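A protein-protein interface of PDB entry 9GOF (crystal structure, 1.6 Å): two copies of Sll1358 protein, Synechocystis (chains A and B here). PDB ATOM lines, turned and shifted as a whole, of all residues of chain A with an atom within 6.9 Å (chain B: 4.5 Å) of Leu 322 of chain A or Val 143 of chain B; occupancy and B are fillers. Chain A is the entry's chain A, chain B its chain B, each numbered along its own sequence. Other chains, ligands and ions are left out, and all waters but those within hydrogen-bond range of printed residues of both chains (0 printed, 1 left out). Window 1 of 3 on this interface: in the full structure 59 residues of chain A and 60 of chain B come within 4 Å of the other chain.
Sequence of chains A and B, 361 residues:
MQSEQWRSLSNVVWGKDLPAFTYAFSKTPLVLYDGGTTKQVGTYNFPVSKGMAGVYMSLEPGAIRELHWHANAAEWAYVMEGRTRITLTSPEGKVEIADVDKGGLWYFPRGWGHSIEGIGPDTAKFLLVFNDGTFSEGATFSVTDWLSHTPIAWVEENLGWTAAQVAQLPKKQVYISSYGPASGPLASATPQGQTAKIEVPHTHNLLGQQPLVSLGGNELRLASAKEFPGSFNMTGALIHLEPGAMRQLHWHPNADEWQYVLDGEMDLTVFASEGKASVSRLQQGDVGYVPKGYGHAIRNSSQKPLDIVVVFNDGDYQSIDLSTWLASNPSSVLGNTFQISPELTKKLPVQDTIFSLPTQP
Of the printed residues of chain B, Leu 322 of chain A touches Val 143 and Leu 147.
Val 143 of chain B touches just these residues of chain A: Leu 322 (3.7 Å), Trp 325 (3.7 Å), Thr 337 (3.6 Å) and Phe 338 (3.7 Å).
Of the printed residues of chain B, Trp 251 of chain A touches Trp 146 (3.8 Å).
Printed residues of chain B within 4 Å of Phe 338 of chain A: Val 143, Thr 144 and Leu 147.
The nearest printed residue of chain B that does not touch Leu 322 of chain A is Trp 146 of chain B (4.01 Å).
The nearest printed residue of chain A that does not touch Phe 141 of chain B is Trp 325 of chain A (4.9 Å).
The side-chain hydroxyl (OG) of Ser 142 of chain B lies within hydrogen-bond range of the side-chain hydroxyl (OG1) of Thr 144 of chain B, 3.0 Å away.
The backbone carbonyl oxygen of Gln 248 of chain A sits at hydrogen-bond distance from a ring nitrogen (ND1) of His 250 of chain A (2.8 Å).
OE2 of Glu 66 of chain B lies within hydrogen-bond range of OG of Ser 142 of chain B (2.6 Å).
The backbone NH (N) of Ile 320 of chain A lies within hydrogen-bond range of the backbone carbonyl oxygen (O) of Trp 251 of chain A, at 3.0 Å.
OE1 of Glu 66 of chain B sits at hydrogen-bond distance from OG1 of Thr 144 of chain B, at 2.7 Å.
O of Leu 249 of chain A lies within hydrogen-bond range of N of Leu 322 of chain A, at 2.9 Å.
No position is printed for both chains.
Of the 20 pairs that touch across the chains among the printed residues, none has its exchanged pair printed and touching as well.
Among the printed residues, pairs that only touch across the chains: Thr 337 of chain A with Thr 144 of chain B (3.4 Å), Phe 271 of chain A with Trp 146 of chain B (3.4 Å), Phe 271 of chain A with Asp 145 of chain B (3.5 Å), Trp 325 of chain A with Leu 67 of chain B (3.5 Å), His 250 of chain A with Trp 146 of chain B (3.5 Å), Phe 271 of chain A with Phe 141 of chain B (3.5 Å), Thr 337 of chain A with Val 143 of chain B (3.6 Å), Leu 249 of chain A with Trp 146 of chain B (3.6 Å), Pro 349 of chain A with Leu 159 of chain B (3.6 Å), Leu 322 of chain A with Val 143 of chain B (3.7 Å), Thr 337 of chain A with Leu 67 of chain B (3.7 Å), Leu 322 of chain A with Leu 147 of chain B (3.7 Å), Thr 337 of chain A with Glu 66 of chain B (3.7 Å), Trp 325 of chain A with Val 143 of chain B (3.7 Å), Phe 338 of chain A with Val 143 of chain B (3.7 Å), Phe 338 of chain A with Thr 144 of chain B (3.8 Å), Phe 271 of chain A with Ser 142 of chain B (3.8 Å), Phe 338 of chain A with Leu 147 of chain B (3.8 Å), Trp 251 of chain A with Trp 146 of chain B (3.8 Å) and Leu 249 of chain A with Leu 147 of chain B (3.97 Å).
Printed residues of chain A that touch a printed residue of chain B: Leu 249, His 250, Trp 251, Phe 271, Leu 322, Trp 325, Thr 337, Phe 338 and Pro 349.
Hydrophobic or aromatic side chains of chain A within 4 Å of the printed part of chain B: Leu 249, Trp 251, Phe 271, Leu 322, Trp 325, Phe 338 and Pro 349.
Printed residues of chain B that touch a printed residue of chain A: Glu 66, Leu 67, Phe 141, Ser 142, Val 143, Thr 144, Asp 145, Trp 146, Leu 147 and Leu 159.
Among the printed residues, 20 pairs touch across the chains.
Among the printed residues, no Asp or Glu carboxylate lies within 4 Å of a Lys or Arg side-chain nitrogen of the other chain.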
ATOM      1  N   GLN A 248       7.292 -12.355 -31.365  1.00  0.00           N
ATOM      2  CA  GLN A 248       8.546 -11.690 -31.024  1.00  0.00           C
ATOM      3  C   GLN A 248       8.643 -11.304 -29.557  1.00  0.00           C
ATOM      4  O   GLN A 248       7.645 -11.145 -28.846  1.00  0.00           O
ATOM      5  CB  GLN A 248       8.738 -10.428 -31.872  1.00  0.00           C
ATOM      6  CG  GLN A 248       8.803 -10.666 -33.364  1.00  0.00           C
ATOM      7  CD  GLN A 248       9.335  -9.432 -34.085  1.00  0.00           C
ATOM      8  OE1 GLN A 248       9.739  -8.457 -33.446  1.00  0.00           O
ATOM      9  NE2 GLN A 248       9.386  -9.491 -35.412  1.00  0.00           N
ATOM     10  N   LEU A 249       9.895 -11.129 -29.132  1.00  0.00           N
ATOM     11  CA  LEU A 249      10.232 -10.605 -27.812  1.00  0.00           C
ATOM     12  C   LEU A 249       9.565  -9.259 -27.562  1.00  0.00           C
ATOM     13  O   LEU A 249       9.652  -8.349 -28.392  1.00  0.00           O
ATOM     14  CB  LEU A 249      11.751 -10.447 -27.714  1.00  0.00           C
ATOM     15  CG  LEU A 249      12.519 -11.762 -27.665  1.00  0.00           C
ATOM     16  CD1 LEU A 249      13.966 -11.557 -28.155  1.00  0.00           C
ATOM     17  CD2 LEU A 249      12.490 -12.301 -26.240  1.00  0.00           C
ATOM     18  N   HIS A 250       8.929  -9.124 -26.400  1.00  0.00           N
ATOM     19  CA  HIS A 250       8.213  -7.898 -26.062  1.00  0.00           C
ATOM     20  C   HIS A 250       7.969  -7.870 -24.560  1.00  0.00           C
ATOM     21  O   HIS A 250       8.227  -8.846 -23.850  1.00  0.00           O
ATOM     22  CB  HIS A 250       6.887  -7.795 -26.830  1.00  0.00           C
ATOM     23  CG  HIS A 250       5.872  -8.825 -26.433  1.00  0.00           C
ATOM     24  ND1 HIS A 250       5.921 -10.131 -26.876  1.00  0.00           N
ATOM     25  CD2 HIS A 250       4.769  -8.732 -25.650  1.00  0.00           C
ATOM     26  CE1 HIS A 250       4.893 -10.802 -26.377  1.00  0.00           C
ATOM     27  NE2 HIS A 250       4.179  -9.975 -25.632  1.00  0.00           N
ATOM     28  N   TRP A 251       7.450  -6.734 -24.081  1.00  0.00           N
ATOM     29  CA  TRP A 251       6.891  -6.675 -22.738  1.00  0.00           C
ATOM     30  C   TRP A 251       5.637  -5.814 -22.749  1.00  0.00           C
ATOM     31  O   TRP A 251       5.375  -5.069 -23.699  1.00  0.00           O
ATOM     32  CB  TRP A 251       7.897  -6.141 -21.705  1.00  0.00           C
ATOM     33  CG  TRP A 251       8.160  -4.647 -21.744  1.00  0.00           C
ATOM     34  CD1 TRP A 251       7.518  -3.674 -21.020  1.00  0.00           C
ATOM     35  CD2 TRP A 251       9.167  -3.974 -22.517  1.00  0.00           C
ATOM     36  NE1 TRP A 251       8.054  -2.436 -21.312  1.00  0.00           N
ATOM     37  CE2 TRP A 251       9.069  -2.594 -22.223  1.00  0.00           C
ATOM     38  CE3 TRP A 251      10.142  -4.406 -23.429  1.00  0.00           C
ATOM     39  CZ2 TRP A 251       9.908  -1.642 -22.815  1.00  0.00           C
ATOM     40  CZ3 TRP A 251      10.968  -3.463 -24.021  1.00  0.00           C
ATOM     41  CH2 TRP A 251      10.850  -2.096 -23.705  1.00  0.00           C
ATOM     42  N   PHE A 271      11.818 -13.391 -19.110  1.00  0.00           N
ATOM     43  CA  PHE A 271      12.997 -12.690 -18.605  1.00  0.00           C
ATOM     44  C   PHE A 271      12.573 -11.785 -17.451  1.00  0.00           C
ATOM     45  O   PHE A 271      11.691 -10.933 -17.615  1.00  0.00           O
ATOM     46  CB  PHE A 271      13.655 -11.880 -19.723  1.00  0.00           C
ATOM     47  CG  PHE A 271      14.670 -10.892 -19.229  1.00  0.00           C
ATOM     48  CD1 PHE A 271      15.804 -11.333 -18.561  1.00  0.00           C
ATOM     49  CD2 PHE A 271      14.490  -9.531 -19.429  1.00  0.00           C
ATOM     50  CE1 PHE A 271      16.744 -10.433 -18.083  1.00  0.00           C
ATOM     51  CE2 PHE A 271      15.433  -8.623 -18.959  1.00  0.00           C
ATOM     52  CZ  PHE A 271      16.556  -9.081 -18.288  1.00  0.00           C
ATOM     53  N   ILE A 320       5.452  -3.323 -26.101  1.00  0.00           N
ATOM     54  CA  ILE A 320       6.641  -2.775 -26.740  1.00  0.00           C
ATOM     55  C   ILE A 320       7.444  -3.973 -27.208  1.00  0.00           C
ATOM     56  O   ILE A 320       7.940  -4.751 -26.384  1.00  0.00           O
ATOM     57  CB  ILE A 320       7.457  -1.874 -25.801  1.00  0.00           C
ATOM     58  CG1 ILE A 320       6.596  -0.681 -25.365  1.00  0.00           C
ATOM     59  CG2 ILE A 320       8.745  -1.391 -26.501  1.00  0.00           C
ATOM     60  CD1 ILE A 320       7.311   0.315 -24.499  1.00  0.00           C
ATOM     61  N   ASP A 321       7.501  -4.163 -28.520  1.00  0.00           N
ATOM     62  CA  ASP A 321       8.341  -5.203 -29.096  1.00  0.00           C
ATOM     63  C   ASP A 321       9.787  -4.749 -29.112  1.00  0.00           C
ATOM     64  O   ASP A 321      10.083  -3.577 -29.361  1.00  0.00           O
ATOM     65  CB  ASP A 321       7.904  -5.545 -30.522  1.00  0.00           C
ATOM     66  CG  ASP A 321       6.571  -6.280 -30.567  1.00  0.00           C
ATOM     67  OD1 ASP A 321       6.361  -7.195 -29.766  1.00  0.00           O
ATOM     68  OD2 ASP A 321       5.719  -5.924 -31.407  1.00  0.00           O
ATOM     69  N   LEU A 322      10.694  -5.694 -28.860  1.00  0.00           N
ATOM     70  CA  LEU A 322      12.118  -5.400 -28.983  1.00  0.00           C
ATOM     71  C   LEU A 322      12.437  -4.740 -30.321  1.00  0.00           C
ATOM     72  O   LEU A 322      13.195  -3.758 -30.377  1.00  0.00           O
ATOM     73  CB  LEU A 322      12.917  -6.696 -28.828  1.00  0.00           C
ATOM     74  CG  LEU A 322      14.422  -6.596 -29.112  1.00  0.00           C
ATOM     75  CD1 LEU A 322      15.123  -5.948 -27.937  1.00  0.00           C
ATOM     76  CD2 LEU A 322      14.971  -7.983 -29.387  1.00  0.00           C
ATOM     77  N   SER A 323      11.853  -5.254 -31.410  1.00  0.00           N
ATOM     78  CA  SER A 323      12.160  -4.728 -32.737  1.00  0.00           C
ATOM     79  C   SER A 323      11.770  -3.257 -32.853  1.00  0.00           C
ATOM     80  O   SER A 323      12.561  -2.433 -33.330  1.00  0.00           O
ATOM     81  CB  SER A 323      11.449  -5.554 -33.806  1.00  0.00           C
ATOM     82  OG  SER A 323      10.071  -5.646 -33.490  1.00  0.00           O
ATOM     83  N   THR A 324      10.547  -2.916 -32.435  1.00  0.00           N
ATOM     84  CA  THR A 324      10.124  -1.515 -32.398  1.00  0.00           C
ATOM     85  C   THR A 324      11.104  -0.672 -31.602  1.00  0.00           C
ATOM     86  O   THR A 324      11.527   0.407 -32.038  1.00  0.00           O
ATOM     87  CB  THR A 324       8.740  -1.405 -31.764  1.00  0.00           C
ATOM     88  OG1 THR A 324       7.789  -2.040 -32.617  1.00  0.00           O
ATOM     89  CG2 THR A 324       8.359   0.073 -31.566  1.00  0.00           C
ATOM     90  N   TRP A 325      11.467  -1.161 -30.414  1.00  0.00           N
ATOM     91  CA  TRP A 325      12.335  -0.406 -29.519  1.00  0.00           C
ATOM     92  C   TRP A 325      13.694  -0.146 -30.152  1.00  0.00           C
ATOM     93  O   TRP A 325      14.190   0.989 -30.148  1.00  0.00           O
ATOM     94  CB  TRP A 325      12.495  -1.175 -28.211  1.00  0.00           C
ATOM     95  CG  TRP A 325      13.118  -0.402 -27.096  1.00  0.00           C
ATOM     96  CD1 TRP A 325      13.197   0.965 -26.964  1.00  0.00           C
ATOM     97  CD2 TRP A 325      13.731  -0.957 -25.930  1.00  0.00           C
ATOM     98  NE1 TRP A 325      13.826   1.284 -25.782  1.00  0.00           N
ATOM     99  CE2 TRP A 325      14.166   0.124 -25.132  1.00  0.00           C
ATOM    100  CE3 TRP A 325      13.961  -2.269 -25.488  1.00  0.00           C
ATOM    101  CZ2 TRP A 325      14.807  -0.065 -23.912  1.00  0.00           C
ATOM    102  CZ3 TRP A 325      14.602  -2.459 -24.273  1.00  0.00           C
ATOM    103  CH2 TRP A 325      15.024  -1.361 -23.501  1.00  0.00           C
ATOM    104  N   LEU A 326      14.323  -1.189 -30.692  1.00  0.00           N
ATOM    105  CA  LEU A 326      15.647  -0.990 -31.280  1.00  0.00           C
ATOM    106  C   LEU A 326      15.562  -0.143 -32.546  1.00  0.00           C
ATOM    107  O   LEU A 326      16.440   0.690 -32.802  1.00  0.00           O
ATOM    108  CB  LEU A 326      16.296  -2.343 -31.566  1.00  0.00           C
ATOM    109  CG  LEU A 326      16.502  -3.240 -30.340  1.00  0.00           C
ATOM    110  CD1 LEU A 326      17.436  -4.405 -30.695  1.00  0.00           C
ATOM    111  CD2 LEU A 326      17.048  -2.469 -29.127  1.00  0.00           C
ATOM    112  N   ALA A 327      14.499  -0.317 -33.338  1.00  0.00           N
ATOM    113  CA  ALA A 327      14.368   0.487 -34.549  1.00  0.00           C
ATOM    114  C   ALA A 327      14.211   1.970 -34.226  1.00  0.00           C
ATOM    115  O   ALA A 327      14.593   2.825 -35.034  1.00  0.00           O
ATOM    116  CB  ALA A 327      13.178   0.007 -35.380  1.00  0.00           C
ATOM    117  N   SER A 328      13.642   2.293 -33.061  1.00  0.00           N
ATOM    118  CA  SER A 328      13.406   3.683 -32.688  1.00  0.00           C
ATOM    119  C   SER A 328      14.672   4.401 -32.236  1.00  0.00           C
ATOM    120  O   SER A 328      14.639   5.628 -32.069  1.00  0.00           O
ATOM    121  CB  SER A 328      12.354   3.762 -31.575  1.00  0.00           C
ATOM    122  OG  SER A 328      12.882   3.345 -30.319  1.00  0.00           O
ATOM    123  N   THR A 337      25.287   0.570 -26.464  1.00  0.00           N
ATOM    124  CA  THR A 337      24.584  -0.340 -25.568  1.00  0.00           C
ATOM    125  C   THR A 337      25.044  -1.780 -25.769  1.00  0.00           C
ATOM    126  O   THR A 337      25.375  -2.483 -24.806  1.00  0.00           O
ATOM    127  CB  THR A 337      23.073  -0.234 -25.801  1.00  0.00           C
ATOM    128  OG1 THR A 337      22.606   1.030 -25.311  1.00  0.00           O
ATOM    129  CG2 THR A 337      22.336  -1.369 -25.084  1.00  0.00           C
ATOM    130  N   PHE A 338      25.041  -2.246 -27.014  1.00  0.00           N
ATOM    131  CA  PHE A 338      25.349  -3.642 -27.290  1.00  0.00           C
ATOM    132  C   PHE A 338      26.838  -3.896 -27.455  1.00  0.00           C
ATOM    133  O   PHE A 338      27.245  -5.059 -27.529  1.00  0.00           O
ATOM    134  CB  PHE A 338      24.599  -4.116 -28.540  1.00  0.00           C
ATOM    135  CG  PHE A 338      23.107  -4.246 -28.329  1.00  0.00           C
ATOM    136  CD1 PHE A 338      22.599  -5.228 -27.486  1.00  0.00           C
ATOM    137  CD2 PHE A 338      22.221  -3.391 -28.971  1.00  0.00           C
ATOM    138  CE1 PHE A 338      21.227  -5.356 -27.280  1.00  0.00           C
ATOM    139  CE2 PHE A 338      20.842  -3.513 -28.770  1.00  0.00           C
ATOM    140  CZ  PHE A 338      20.345  -4.493 -27.929  1.00  0.00           C
ATOM    141  N   PRO A 349      17.131  -4.390 -35.925  1.00  0.00           N
ATOM    142  CA  PRO A 349      15.816  -4.261 -36.572  1.00  0.00           C
ATOM    143  C   PRO A 349      15.505  -2.833 -37.002  1.00  0.00           C
ATOM    144  O   PRO A 349      15.836  -1.866 -36.312  1.00  0.00           O
ATOM    145  CB  PRO A 349      14.841  -4.728 -35.484  1.00  0.00           C
ATOM    146  CG  PRO A 349      15.646  -5.690 -34.660  1.00  0.00           C
ATOM    147  CD  PRO A 349      17.035  -5.103 -34.633  1.00  0.00           C
ATOM    148  N   ASP A 352       8.955  -3.681 -37.225  1.00  0.00           N
ATOM    149  CA  ASP A 352       8.361  -4.637 -36.297  1.00  0.00           C
ATOM    150  C   ASP A 352       7.258  -5.403 -37.018  1.00  0.00           C
ATOM    151  O   ASP A 352       6.211  -4.827 -37.340  1.00  0.00           O
ATOM    152  CB  ASP A 352       7.808  -3.908 -35.071  1.00  0.00           C
ATOM    153  CG  ASP A 352       7.088  -4.828 -34.111  1.00  0.00           C
ATOM    154  OD1 ASP A 352       7.296  -6.061 -34.161  1.00  0.00           O
ATOM    155  OD2 ASP A 352       6.321  -4.298 -33.279  1.00  0.00           O
ATOM    156  N   GLU B  66      22.418   2.278 -20.419  1.00  0.00           N
ATOM    157  CA  GLU B  66      21.945   1.503 -21.563  1.00  0.00           C
ATOM    158  C   GLU B  66      20.419   1.456 -21.620  1.00  0.00           C
ATOM    159  O   GLU B  66      19.724   1.699 -20.639  1.00  0.00           O
ATOM    160  CB  GLU B  66      22.468   0.072 -21.499  1.00  0.00           C
ATOM    161  CG  GLU B  66      21.903  -0.702 -20.313  1.00  0.00           C
ATOM    162  CD  GLU B  66      22.015  -2.218 -20.472  1.00  0.00           C
ATOM    163  OE1 GLU B  66      22.053  -2.722 -21.615  1.00  0.00           O
ATOM    164  OE2 GLU B  66      22.107  -2.907 -19.439  1.00  0.00           O
ATOM    165  N   LEU B  67      19.914   1.106 -22.794  1.00  0.00           N
ATOM    166  CA  LEU B  67      18.488   0.881 -23.001  1.00  0.00           C
ATOM    167  C   LEU B  67      17.925  -0.077 -21.958  1.00  0.00           C
ATOM    168  O   LEU B  67      18.420  -1.200 -21.796  1.00  0.00           O
ATOM    169  CB  LEU B  67      18.276   0.332 -24.411  1.00  0.00           C
ATOM    170  CG  LEU B  67      18.522   1.328 -25.544  1.00  0.00           C
ATOM    171  CD1 LEU B  67      18.710   0.575 -26.853  1.00  0.00           C
ATOM    172  CD2 LEU B  67      17.340   2.326 -25.648  1.00  0.00           C
ATOM    173  N   PHE B 141      15.152  -3.604 -16.058  1.00  0.00           N
ATOM    174  CA  PHE B 141      15.127  -4.596 -17.127  1.00  0.00           C
ATOM    175  C   PHE B 141      16.026  -4.107 -18.254  1.00  0.00           C
ATOM    176  O   PHE B 141      15.676  -3.169 -18.975  1.00  0.00           O
ATOM    177  CB  PHE B 141      13.689  -4.828 -17.590  1.00  0.00           C
ATOM    178  CG  PHE B 141      12.886  -5.661 -16.627  1.00  0.00           C
ATOM    179  CD1 PHE B 141      12.443  -5.120 -15.431  1.00  0.00           C
ATOM    180  CD2 PHE B 141      12.615  -7.004 -16.896  1.00  0.00           C
ATOM    181  CE1 PHE B 141      11.721  -5.899 -14.523  1.00  0.00           C
ATOM    182  CE2 PHE B 141      11.898  -7.790 -15.996  1.00  0.00           C
ATOM    183  CZ  PHE B 141      11.446  -7.231 -14.812  1.00  0.00           C
ATOM    184  N   SER B 142      17.185  -4.747 -18.389  1.00  0.00           N
ATOM    185  CA  SER B 142      18.251  -4.336 -19.295  1.00  0.00           C
ATOM    186  C   SER B 142      18.118  -5.063 -20.626  1.00  0.00           C
ATOM    187  O   SER B 142      17.884  -6.273 -20.655  1.00  0.00           O
ATOM    188  CB  SER B 142      19.598  -4.662 -18.640  1.00  0.00           C
ATOM    189  OG  SER B 142      20.586  -5.017 -19.593  1.00  0.00           O
ATOM    190  N   VAL B 143      18.279  -4.330 -21.736  1.00  0.00           N
ATOM    191  CA  VAL B 143      18.143  -4.991 -23.034  1.00  0.00           C
ATOM    192  C   VAL B 143      19.292  -5.970 -23.275  1.00  0.00           C
ATOM    193  O   VAL B 143      19.109  -6.997 -23.941  1.00  0.00           O
ATOM    194  CB  VAL B 143      18.025  -3.958 -24.173  1.00  0.00           C
ATOM    195  CG1 VAL B 143      19.381  -3.330 -24.505  1.00  0.00           C
ATOM    196  CG2 VAL B 143      17.443  -4.618 -25.414  1.00  0.00           C
ATOM    197  N   THR B 144      20.487  -5.685 -22.747  1.00  0.00           N
ATOM    198  CA  THR B 144      21.603  -6.609 -22.928  1.00  0.00           C
ATOM    199  C   THR B 144      21.462  -7.828 -22.021  1.00  0.00           C
ATOM    200  O   THR B 144      21.774  -8.951 -22.437  1.00  0.00           O
ATOM    201  CB  THR B 144      22.932  -5.895 -22.680  1.00  0.00           C
ATOM    202  OG1 THR B 144      22.906  -5.245 -21.401  1.00  0.00           O
ATOM    203  CG2 THR B 144      23.192  -4.862 -23.784  1.00  0.00           C
ATOM    204  N   ASP B 145      20.984  -7.622 -20.790  1.00  0.00           N
ATOM    205  CA  ASP B 145      20.586  -8.742 -19.935  1.00  0.00           C
ATOM    206  C   ASP B 145      19.526  -9.595 -20.631  1.00  0.00           C
ATOM    207  O   ASP B 145      19.620 -10.826 -20.664  1.00  0.00           O
ATOM    208  CB  ASP B 145      20.077  -8.183 -18.594  1.00  0.00           C
ATOM    209  CG  ASP B 145      20.115  -9.198 -17.451  1.00  0.00           C
ATOM    210  OD1 ASP B 145      20.796 -10.243 -17.562  1.00  0.00           O
ATOM    211  OD2 ASP B 145      19.465  -8.919 -16.417  1.00  0.00           O
ATOM    212  N   TRP B 146      18.527  -8.944 -21.232  1.00  0.00           N
ATOM    213  CA  TRP B 146      17.439  -9.652 -21.907  1.00  0.00           C
ATOM    214  C   TRP B 146      17.960 -10.585 -22.992  1.00  0.00           C
ATOM    215  O   TRP B 146      17.631 -11.777 -23.013  1.00  0.00           O
ATOM    216  CB  TRP B 146      16.476  -8.638 -22.522  1.00  0.00           C
ATOM    217  CG  TRP B 146      15.149  -9.188 -22.921  1.00  0.00           C
ATOM    218  CD1 TRP B 146      14.656 -10.451 -22.690  1.00  0.00           C
ATOM    219  CD2 TRP B 146      14.121  -8.473 -23.611  1.00  0.00           C
ATOM    220  NE1 TRP B 146      13.365 -10.552 -23.195  1.00  0.00           N
ATOM    221  CE2 TRP B 146      13.023  -9.349 -23.765  1.00  0.00           C
ATOM    222  CE3 TRP B 146      14.024  -7.168 -24.113  1.00  0.00           C
ATOM    223  CZ2 TRP B 146      11.845  -8.961 -24.400  1.00  0.00           C
ATOM    224  CZ3 TRP B 146      12.847  -6.781 -24.746  1.00  0.00           C
ATOM    225  CH2 TRP B 146      11.773  -7.675 -24.878  1.00  0.00           C
ATOM    226  N   LEU B 147      18.762 -10.056 -23.921  1.00  0.00           N
ATOM    227  CA  LEU B 147      19.141 -10.867 -25.070  1.00  0.00           C
ATOM    228  C   LEU B 147      20.152 -11.947 -24.700  1.00  0.00           C
ATOM    229  O   LEU B 147      20.210 -12.974 -25.380  1.00  0.00           O
ATOM    230  CB  LEU B 147      19.673  -9.977 -26.193  1.00  0.00           C
ATOM    231  CG  LEU B 147      18.632  -9.016 -26.798  1.00  0.00           C
ATOM    232  CD1 LEU B 147      19.131  -8.440 -28.118  1.00  0.00           C
ATOM    233  CD2 LEU B 147      17.270  -9.691 -26.993  1.00  0.00           C
ATOM    234  N   LEU B 159      15.896 -11.557 -34.727  1.00  0.00           N
ATOM    235  CA  LEU B 159      16.695 -10.515 -35.357  1.00  0.00           C
ATOM    236  C   LEU B 159      17.012 -10.811 -36.813  1.00  0.00           C
ATOM    237  O   LEU B 159      17.538  -9.931 -37.508  1.00  0.00           O
ATOM    238  CB  LEU B 159      18.013 -10.316 -34.591  1.00  0.00           C
ATOM    239  CG  LEU B 159      17.923  -9.856 -33.133  1.00  0.00           C
ATOM    240  CD1 LEU B 159      19.318  -9.628 -32.579  1.00  0.00           C
ATOM    241  CD2 LEU B 159      17.094  -8.585 -33.036  1.00  0.00           C
